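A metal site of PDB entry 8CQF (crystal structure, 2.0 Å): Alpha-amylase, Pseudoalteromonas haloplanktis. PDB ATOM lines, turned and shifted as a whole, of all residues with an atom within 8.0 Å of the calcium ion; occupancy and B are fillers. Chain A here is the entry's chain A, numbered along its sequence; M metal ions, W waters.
The backbone carbonyl oxygen of Val 134 lies within hydrogen-bond range of a ring nitrogen (ND1) of His 178 (2.9 Å). The backbone NH (N) of Leu 145 lies within hydrogen-bond range of the backbone carbonyl oxygen (O) of Asn 88. ND1 of His 89 is in hydrogen-bond range of ND2 of Asn 88, 3.0 Å away. The backbone NH (N) of His 117 lies within hydrogen-bond range of the backbone carbonyl oxygen (O) of Asp 144 (2.9 Å). The side-chain amide nitrogen (NE2) of Gln 135 is in hydrogen-bond range of the backbone carbonyl oxygen (O) of Val 179 (3.5 Å). The backbone carbonyl oxygen (O) of Lys 177 sits at hydrogen-bond distance from the side-chain amide nitrogen (NE2) of Gln 135 (3.1 Å).
Within 4 Å of the calcium ion: Asn 88, Gln 135, Asp 144 and His 178. The nearest printed residue that does not touch the calcium ion is Asn 136 (4.3 Å).
The calcium ion is bound by water W2 (2.3 Å), water W1 (2.3 Å), O of His 178 (2.4 Å), OD1 of Asn 88 (2.4 Å), water W3 (2.4 Å), OD2 of Asp 144 (2.4 Å), O of Gln 135 (2.5 Å) and OD1 of Asp 144 (2.6 Å). The calcium ion has eight donor atoms within binding distance.
Water W1 bridges the backbone carbonyl oxygen of Asn 88 (2.6 Å) and the backbone carbonyl oxygen of Leu 145 (2.8 Å).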
ATOM      1  N   ILE A  87       3.278  16.500  16.644  1.00  0.00           N
ATOM      2  CA  ILE A  87       3.732  15.805  15.443  1.00  0.00           C
ATOM      3  C   ILE A  87       3.015  14.484  15.196  1.00  0.00           C
ATOM      4  O   ILE A  87       3.164  13.897  14.104  1.00  0.00           O
ATOM      5  CB  ILE A  87       5.245  15.534  15.459  1.00  0.00           C
ATOM      6  CG1 ILE A  87       5.623  14.640  16.635  1.00  0.00           C
ATOM      7  CG2 ILE A  87       6.023  16.842  15.526  1.00  0.00           C
ATOM      8  CD1 ILE A  87       7.043  14.133  16.592  1.00  0.00           C
ATOM      9  N   ASN A  88       2.240  13.988  16.155  1.00  0.00           N
ATOM     10  CA  ASN A  88       1.695  12.645  16.080  1.00  0.00           C
ATOM     11  C   ASN A  88       0.248  12.591  15.573  1.00  0.00           C
ATOM     12  O   ASN A  88      -0.142  11.548  15.024  1.00  0.00           O
ATOM     13  CB  ASN A  88       1.780  11.983  17.468  1.00  0.00           C
ATOM     14  CG  ASN A  88       1.204  10.578  17.464  1.00  0.00           C
ATOM     15  OD1 ASN A  88       1.760   9.678  16.851  1.00  0.00           O
ATOM     16  ND2 ASN A  88       0.068  10.405  18.132  1.00  0.00           N
ATOM     17  N   HIS A  89      -0.533  13.652  15.708  1.00  0.00           N
ATOM     18  CA  HIS A  89      -1.972  13.476  15.561  1.00  0.00           C
ATOM     19  C   HIS A  89      -2.726  14.764  15.352  1.00  0.00           C
ATOM     20  O   HIS A  89      -2.174  15.861  15.456  1.00  0.00           O
ATOM     21  CB  HIS A  89      -2.555  12.750  16.798  1.00  0.00           C
ATOM     22  CG  HIS A  89      -2.235  13.432  18.100  1.00  0.00           C
ATOM     23  ND1 HIS A  89      -1.240  12.999  18.946  1.00  0.00           N
ATOM     24  CD2 HIS A  89      -2.800  14.501  18.717  1.00  0.00           C
ATOM     25  CE1 HIS A  89      -1.179  13.782  20.009  1.00  0.00           C
ATOM     26  NE2 HIS A  89      -2.109  14.708  19.884  1.00  0.00           N
ATOM     27  N   HIS A 117      -3.069   6.900   9.562  1.00  0.00           N
ATOM     28  CA  HIS A 117      -3.105   5.469   9.769  1.00  0.00           C
ATOM     29  C   HIS A 117      -4.542   5.004   9.941  1.00  0.00           C
ATOM     30  O   HIS A 117      -5.407   5.727  10.445  1.00  0.00           O
ATOM     31  CB  HIS A 117      -2.294   5.090  10.991  1.00  0.00           C
ATOM     32  CG  HIS A 117      -0.825   5.362  10.857  1.00  0.00           C
ATOM     33  ND1 HIS A 117      -0.060   5.818  11.896  1.00  0.00           N
ATOM     34  CD2 HIS A 117       0.007   5.237   9.797  1.00  0.00           C
ATOM     35  CE1 HIS A 117       1.197   5.948  11.498  1.00  0.00           C
ATOM     36  NE2 HIS A 117       1.259   5.602  10.218  1.00  0.00           N
ATOM     37  N   ILE A 122      -4.919   2.329  20.775  1.00  0.00           N
ATOM     38  CA  ILE A 122      -3.816   1.953  21.644  1.00  0.00           C
ATOM     39  C   ILE A 122      -4.416   1.468  22.949  1.00  0.00           C
ATOM     40  O   ILE A 122      -5.119   2.231  23.625  1.00  0.00           O
ATOM     41  CB  ILE A 122      -2.852   3.115  21.876  1.00  0.00           C
ATOM     42  CG1 ILE A 122      -2.312   3.659  20.569  1.00  0.00           C
ATOM     43  CG2 ILE A 122      -1.675   2.682  22.750  1.00  0.00           C
ATOM     44  CD1 ILE A 122      -1.503   4.926  20.756  1.00  0.00           C
ATOM     45  N   TYR A 132       4.164  -1.633  17.373  1.00  0.00           N
ATOM     46  CA  TYR A 132       3.417  -1.228  16.187  1.00  0.00           C
ATOM     47  C   TYR A 132       2.136  -0.519  16.568  1.00  0.00           C
ATOM     48  O   TYR A 132       1.781   0.520  15.995  1.00  0.00           O
ATOM     49  CB  TYR A 132       3.111  -2.455  15.290  1.00  0.00           C
ATOM     50  CG  TYR A 132       2.239  -2.118  14.105  1.00  0.00           C
ATOM     51  CD1 TYR A 132       2.787  -1.633  12.930  1.00  0.00           C
ATOM     52  CD2 TYR A 132       0.867  -2.249  14.177  1.00  0.00           C
ATOM     53  CE1 TYR A 132       1.989  -1.306  11.852  1.00  0.00           C
ATOM     54  CE2 TYR A 132       0.066  -1.918  13.116  1.00  0.00           C
ATOM     55  CZ  TYR A 132       0.628  -1.455  11.950  1.00  0.00           C
ATOM     56  OH  TYR A 132      -0.166  -1.112  10.886  1.00  0.00           O
ATOM     57  N   ARG A 133       1.391  -1.065  17.528  1.00  0.00           N
ATOM     58  CA  ARG A 133       0.135  -0.428  17.908  1.00  0.00           C
ATOM     59  C   ARG A 133       0.388   0.918  18.582  1.00  0.00           C
ATOM     60  O   ARG A 133      -0.360   1.871  18.352  1.00  0.00           O
ATOM     61  CB  ARG A 133      -0.665  -1.354  18.804  1.00  0.00           C
ATOM     62  CG  ARG A 133      -1.272  -2.566  18.065  1.00  0.00           C
ATOM     63  CD  ARG A 133      -2.082  -3.426  19.039  1.00  0.00           C
ATOM     64  NE  ARG A 133      -3.392  -2.844  19.290  1.00  0.00           N
ATOM     65  CZ  ARG A 133      -4.381  -2.813  18.404  1.00  0.00           C
ATOM     66  NH1 ARG A 133      -4.221  -3.297  17.178  1.00  0.00           N
ATOM     67  NH2 ARG A 133      -5.553  -2.303  18.748  1.00  0.00           N
ATOM     68  N   VAL A 134       1.455   1.020  19.394  1.00  0.00           N
ATOM     69  CA  VAL A 134       1.751   2.263  20.096  1.00  0.00           C
ATOM     70  C   VAL A 134       1.985   3.388  19.097  1.00  0.00           C
ATOM     71  O   VAL A 134       1.607   4.537  19.321  1.00  0.00           O
ATOM     72  CB  VAL A 134       2.980   2.101  21.007  1.00  0.00           C
ATOM     73  CG1 VAL A 134       3.405   3.461  21.552  1.00  0.00           C
ATOM     74  CG2 VAL A 134       2.714   1.100  22.156  1.00  0.00           C
ATOM     75  N   GLN A 135       2.602   3.062  17.964  1.00  0.00           N
ATOM     76  CA  GLN A 135       2.977   4.089  17.009  1.00  0.00           C
ATOM     77  C   GLN A 135       2.027   4.247  15.819  1.00  0.00           C
ATOM     78  O   GLN A 135       2.109   5.268  15.139  1.00  0.00           O
ATOM     79  CB  GLN A 135       4.399   3.823  16.516  1.00  0.00           C
ATOM     80  CG  GLN A 135       5.392   3.696  17.694  1.00  0.00           C
ATOM     81  CD  GLN A 135       6.870   3.648  17.269  1.00  0.00           C
ATOM     82  OE1 GLN A 135       7.222   3.031  16.259  1.00  0.00           O
ATOM     83  NE2 GLN A 135       7.742   4.292  18.060  1.00  0.00           N
ATOM     84  N   ASN A 136       1.127   3.292  15.570  1.00  0.00           N
ATOM     85  CA  ASN A 136       0.218   3.420  14.444  1.00  0.00           C
ATOM     86  C   ASN A 136      -1.249   3.491  14.841  1.00  0.00           C
ATOM     87  O   ASN A 136      -2.063   3.880  13.998  1.00  0.00           O
ATOM     88  CB  ASN A 136       0.393   2.251  13.453  1.00  0.00           C
ATOM     89  CG  ASN A 136       1.745   2.278  12.785  1.00  0.00           C
ATOM     90  OD1 ASN A 136       1.908   2.838  11.694  1.00  0.00           O
ATOM     91  ND2 ASN A 136       2.745   1.690  13.442  1.00  0.00           N
ATOM     92  N   CYS A 137      -1.601   3.166  16.078  1.00  0.00           N
ATOM     93  CA  CYS A 137      -2.968   3.251  16.556  1.00  0.00           C
ATOM     94  C   CYS A 137      -3.189   4.609  17.223  1.00  0.00           C
ATOM     95  O   CYS A 137      -2.274   5.421  17.342  1.00  0.00           O
ATOM     96  CB  CYS A 137      -3.280   2.100  17.518  1.00  0.00           C
ATOM     97  SG  CYS A 137      -3.363   0.443  16.665  1.00  0.00           S
ATOM     98  N   GLU A 138      -4.408   4.827  17.676  1.00  0.00           N
ATOM     99  CA  GLU A 138      -4.848   6.121  18.130  1.00  0.00           C
ATOM    100  C   GLU A 138      -4.664   6.254  19.628  1.00  0.00           C
ATOM    101  O   GLU A 138      -5.118   5.410  20.411  1.00  0.00           O
ATOM    102  CB  GLU A 138      -6.314   6.339  17.779  1.00  0.00           C
ATOM    103  CG  GLU A 138      -6.488   6.335  16.311  1.00  0.00           C
ATOM    104  CD  GLU A 138      -7.918   6.551  15.919  1.00  0.00           C
ATOM    105  OE1 GLU A 138      -8.801   6.364  16.789  1.00  0.00           O
ATOM    106  OE2 GLU A 138      -8.136   6.901  14.725  1.00  0.00           O
ATOM    107  N   LEU A 139      -3.990   7.334  20.020  1.00  0.00           N
ATOM    108  CA  LEU A 139      -3.853   7.734  21.422  1.00  0.00           C
ATOM    109  C   LEU A 139      -5.138   8.409  21.835  1.00  0.00           C
ATOM    110  O   LEU A 139      -5.462   9.502  21.357  1.00  0.00           O
ATOM    111  CB  LEU A 139      -2.658   8.669  21.556  1.00  0.00           C
ATOM    112  CG  LEU A 139      -2.274   9.188  22.942  1.00  0.00           C
ATOM    113  CD1 LEU A 139      -2.034   8.030  23.919  1.00  0.00           C
ATOM    114  CD2 LEU A 139      -1.042  10.112  22.825  1.00  0.00           C
ATOM    115  N   LEU A 142      -7.319  10.104  19.232  1.00  0.00           N
ATOM    116  CA  LEU A 142      -6.794  11.171  18.392  1.00  0.00           C
ATOM    117  C   LEU A 142      -6.369  10.583  17.037  1.00  0.00           C
ATOM    118  O   LEU A 142      -5.788   9.501  16.985  1.00  0.00           O
ATOM    119  CB  LEU A 142      -5.630  11.835  19.106  1.00  0.00           C
ATOM    120  CG  LEU A 142      -5.962  12.505  20.440  1.00  0.00           C
ATOM    121  CD1 LEU A 142      -4.718  12.675  21.328  1.00  0.00           C
ATOM    122  CD2 LEU A 142      -6.689  13.842  20.223  1.00  0.00           C
ATOM    123  N   ALA A 143      -6.705  11.282  15.967  1.00  0.00           N
ATOM    124  CA  ALA A 143      -6.416  10.781  14.624  1.00  0.00           C
ATOM    125  C   ALA A 143      -4.924  10.664  14.390  1.00  0.00           C
ATOM    126  O   ALA A 143      -4.193  11.660  14.444  1.00  0.00           O
ATOM    127  CB  ALA A 143      -7.031  11.689  13.569  1.00  0.00           C
ATOM    128  N   ASP A 144      -4.461   9.455  14.148  1.00  0.00           N
ATOM    129  CA  ASP A 144      -3.018   9.198  14.105  1.00  0.00           C
ATOM    130  C   ASP A 144      -2.503   9.444  12.695  1.00  0.00           C
ATOM    131  O   ASP A 144      -2.832   8.715  11.749  1.00  0.00           O
ATOM    132  CB  ASP A 144      -2.709   7.787  14.596  1.00  0.00           C
ATOM    133  CG  ASP A 144      -1.284   7.666  15.108  1.00  0.00           C
ATOM    134  OD1 ASP A 144      -0.940   8.354  16.110  1.00  0.00           O
ATOM    135  OD2 ASP A 144      -0.506   6.896  14.503  1.00  0.00           O
ATOM    136  N   LEU A 145      -1.695  10.481  12.547  1.00  0.00           N
ATOM    137  CA  LEU A 145      -1.189  10.863  11.234  1.00  0.00           C
ATOM    138  C   LEU A 145      -0.232   9.806  10.706  1.00  0.00           C
ATOM    139  O   LEU A 145       0.506   9.158  11.444  1.00  0.00           O
ATOM    140  CB  LEU A 145      -0.473  12.215  11.309  1.00  0.00           C
ATOM    141  CG  LEU A 145      -1.301  13.488  11.319  1.00  0.00           C
ATOM    142  CD1 LEU A 145      -0.448  14.618  11.950  1.00  0.00           C
ATOM    143  CD2 LEU A 145      -1.812  13.908   9.931  1.00  0.00           C
ATOM    144  N   ASP A 146      -0.215   9.652   9.385  1.00  0.00           N
ATOM    145  CA  ASP A 146       0.770   8.797   8.726  1.00  0.00           C
ATOM    146  C   ASP A 146       2.088   9.567   8.616  1.00  0.00           C
ATOM    147  O   ASP A 146       2.374  10.227   7.613  1.00  0.00           O
ATOM    148  CB  ASP A 146       0.270   8.353   7.358  1.00  0.00           C
ATOM    149  CG  ASP A 146       1.216   7.383   6.709  1.00  0.00           C
ATOM    150  OD1 ASP A 146       2.154   6.926   7.399  1.00  0.00           O
ATOM    151  OD2 ASP A 146       1.020   7.102   5.490  1.00  0.00           O
ATOM    152  N   THR A 147       2.895   9.459   9.657  1.00  0.00           N
ATOM    153  CA  THR A 147       4.113  10.242   9.744  1.00  0.00           C
ATOM    154  C   THR A 147       5.210   9.690   8.851  1.00  0.00           C
ATOM    155  O   THR A 147       6.283  10.286   8.789  1.00  0.00           O
ATOM    156  CB  THR A 147       4.625  10.304  11.189  1.00  0.00           C
ATOM    157  OG1 THR A 147       4.576   9.024  11.797  1.00  0.00           O
ATOM    158  CG2 THR A 147       3.768  11.279  12.029  1.00  0.00           C
ATOM    159  N   ALA A 175       4.346  13.666  22.311  1.00  0.00           N
ATOM    160  CA  ALA A 175       3.933  12.284  22.034  1.00  0.00           C
ATOM    161  C   ALA A 175       4.920  11.592  21.108  1.00  0.00           C
ATOM    162  O   ALA A 175       4.534  10.763  20.269  1.00  0.00           O
ATOM    163  CB  ALA A 175       2.515  12.256  21.435  1.00  0.00           C
ATOM    164  N   SER A 176       6.214  11.884  21.270  1.00  0.00           N
ATOM    165  CA  SER A 176       7.229  11.319  20.359  1.00  0.00           C
ATOM    166  C   SER A 176       7.284   9.786  20.404  1.00  0.00           C
ATOM    167  O   SER A 176       7.635   9.156  19.403  1.00  0.00           O
ATOM    168  CB  SER A 176       8.591  11.905  20.706  1.00  0.00           C
ATOM    169  OG  SER A 176       8.697  13.206  20.176  1.00  0.00           O
ATOM    170  N   LYS A 177       6.943   9.178  21.540  1.00  0.00           N
ATOM    171  CA  LYS A 177       6.923   7.719  21.624  1.00  0.00           C
ATOM    172  C   LYS A 177       5.984   7.101  20.596  1.00  0.00           C
ATOM    173  O   LYS A 177       6.199   5.960  20.150  1.00  0.00           O
ATOM    174  CB  LYS A 177       6.497   7.281  23.028  1.00  0.00           C
ATOM    175  CG  LYS A 177       6.087   5.822  23.166  1.00  0.00           C
ATOM    176  CD  LYS A 177       6.474   5.237  24.525  1.00  0.00           C
ATOM    177  CE  LYS A 177       5.478   5.542  25.568  1.00  0.00           C
ATOM    178  NZ  LYS A 177       5.895   5.119  26.963  1.00  0.00           N
ATOM    179  N   HIS A 178       4.927   7.822  20.227  1.00  0.00           N
ATOM    180  CA  HIS A 178       3.896   7.332  19.318  1.00  0.00           C
ATOM    181  C   HIS A 178       4.247   7.551  17.871  1.00  0.00           C
ATOM    182  O   HIS A 178       3.430   7.265  16.998  1.00  0.00           O
ATOM    183  CB  HIS A 178       2.570   7.998  19.683  1.00  0.00           C
ATOM    184  CG  HIS A 178       2.173   7.716  21.082  1.00  0.00           C
ATOM    185  ND1 HIS A 178       1.512   6.558  21.458  1.00  0.00           N
ATOM    186  CD2 HIS A 178       2.434   8.383  22.231  1.00  0.00           C
ATOM    187  CE1 HIS A 178       1.340   6.560  22.765  1.00  0.00           C
ATOM    188  NE2 HIS A 178       1.910   7.633  23.261  1.00  0.00           N
ATOM    189  N   VAL A 179       5.475   8.022  17.617  1.00  0.00           N
ATOM    190  CA  VAL A 179       6.022   8.198  16.292  1.00  0.00           C
ATOM    191  C   VAL A 179       7.342   7.430  16.200  1.00  0.00           C
ATOM    192  O   VAL A 179       8.229   7.598  17.039  1.00  0.00           O
ATOM    193  CB  VAL A 179       6.224   9.685  15.986  1.00  0.00           C
ATOM    194  CG1 VAL A 179       6.846   9.880  14.634  1.00  0.00           C
ATOM    195  CG2 VAL A 179       4.872  10.401  16.152  1.00  0.00           C
ATOM    196  N   ALA A 180       7.459   6.555  15.206  1.00  0.00           N
ATOM    197  CA  ALA A 180       8.713   5.844  15.027  1.00  0.00           C
ATOM    198  C   ALA A 180       9.857   6.846  14.934  1.00  0.00           C
ATOM    199  O   ALA A 180       9.751   7.876  14.258  1.00  0.00           O
ATOM    200  CB  ALA A 180       8.669   4.963  13.768  1.00  0.00           C
ATOM    201  N   ASP A 183      10.578   7.921  11.456  1.00  0.00           N
ATOM    202  CA  ASP A 183       9.742   9.000  10.915  1.00  0.00           C
ATOM    203  C   ASP A 183      10.227  10.366  11.403  1.00  0.00           C
ATOM    204  O   ASP A 183      10.209  11.350  10.647  1.00  0.00           O
ATOM    205  CB  ASP A 183       8.286   8.812  11.320  1.00  0.00           C
ATOM    206  CG  ASP A 183       7.645   7.563  10.699  1.00  0.00           C
ATOM    207  OD1 ASP A 183       8.281   6.859   9.898  1.00  0.00           O
ATOM    208  OD2 ASP A 183       6.465   7.306  11.029  1.00  0.00           O
HETATM  209 CA    CA M   1       1.497   7.618  15.699  1.00  0.00          CA
HETATM  210  O   HOH W   1       1.130   9.377  14.215  1.00  0.00           O
HETATM  211  O   HOH W   2       0.605   6.402  17.411  1.00  0.00           O
HETATM  212  O   HOH W   3       3.017   7.543  13.816  1.00  0.00           O
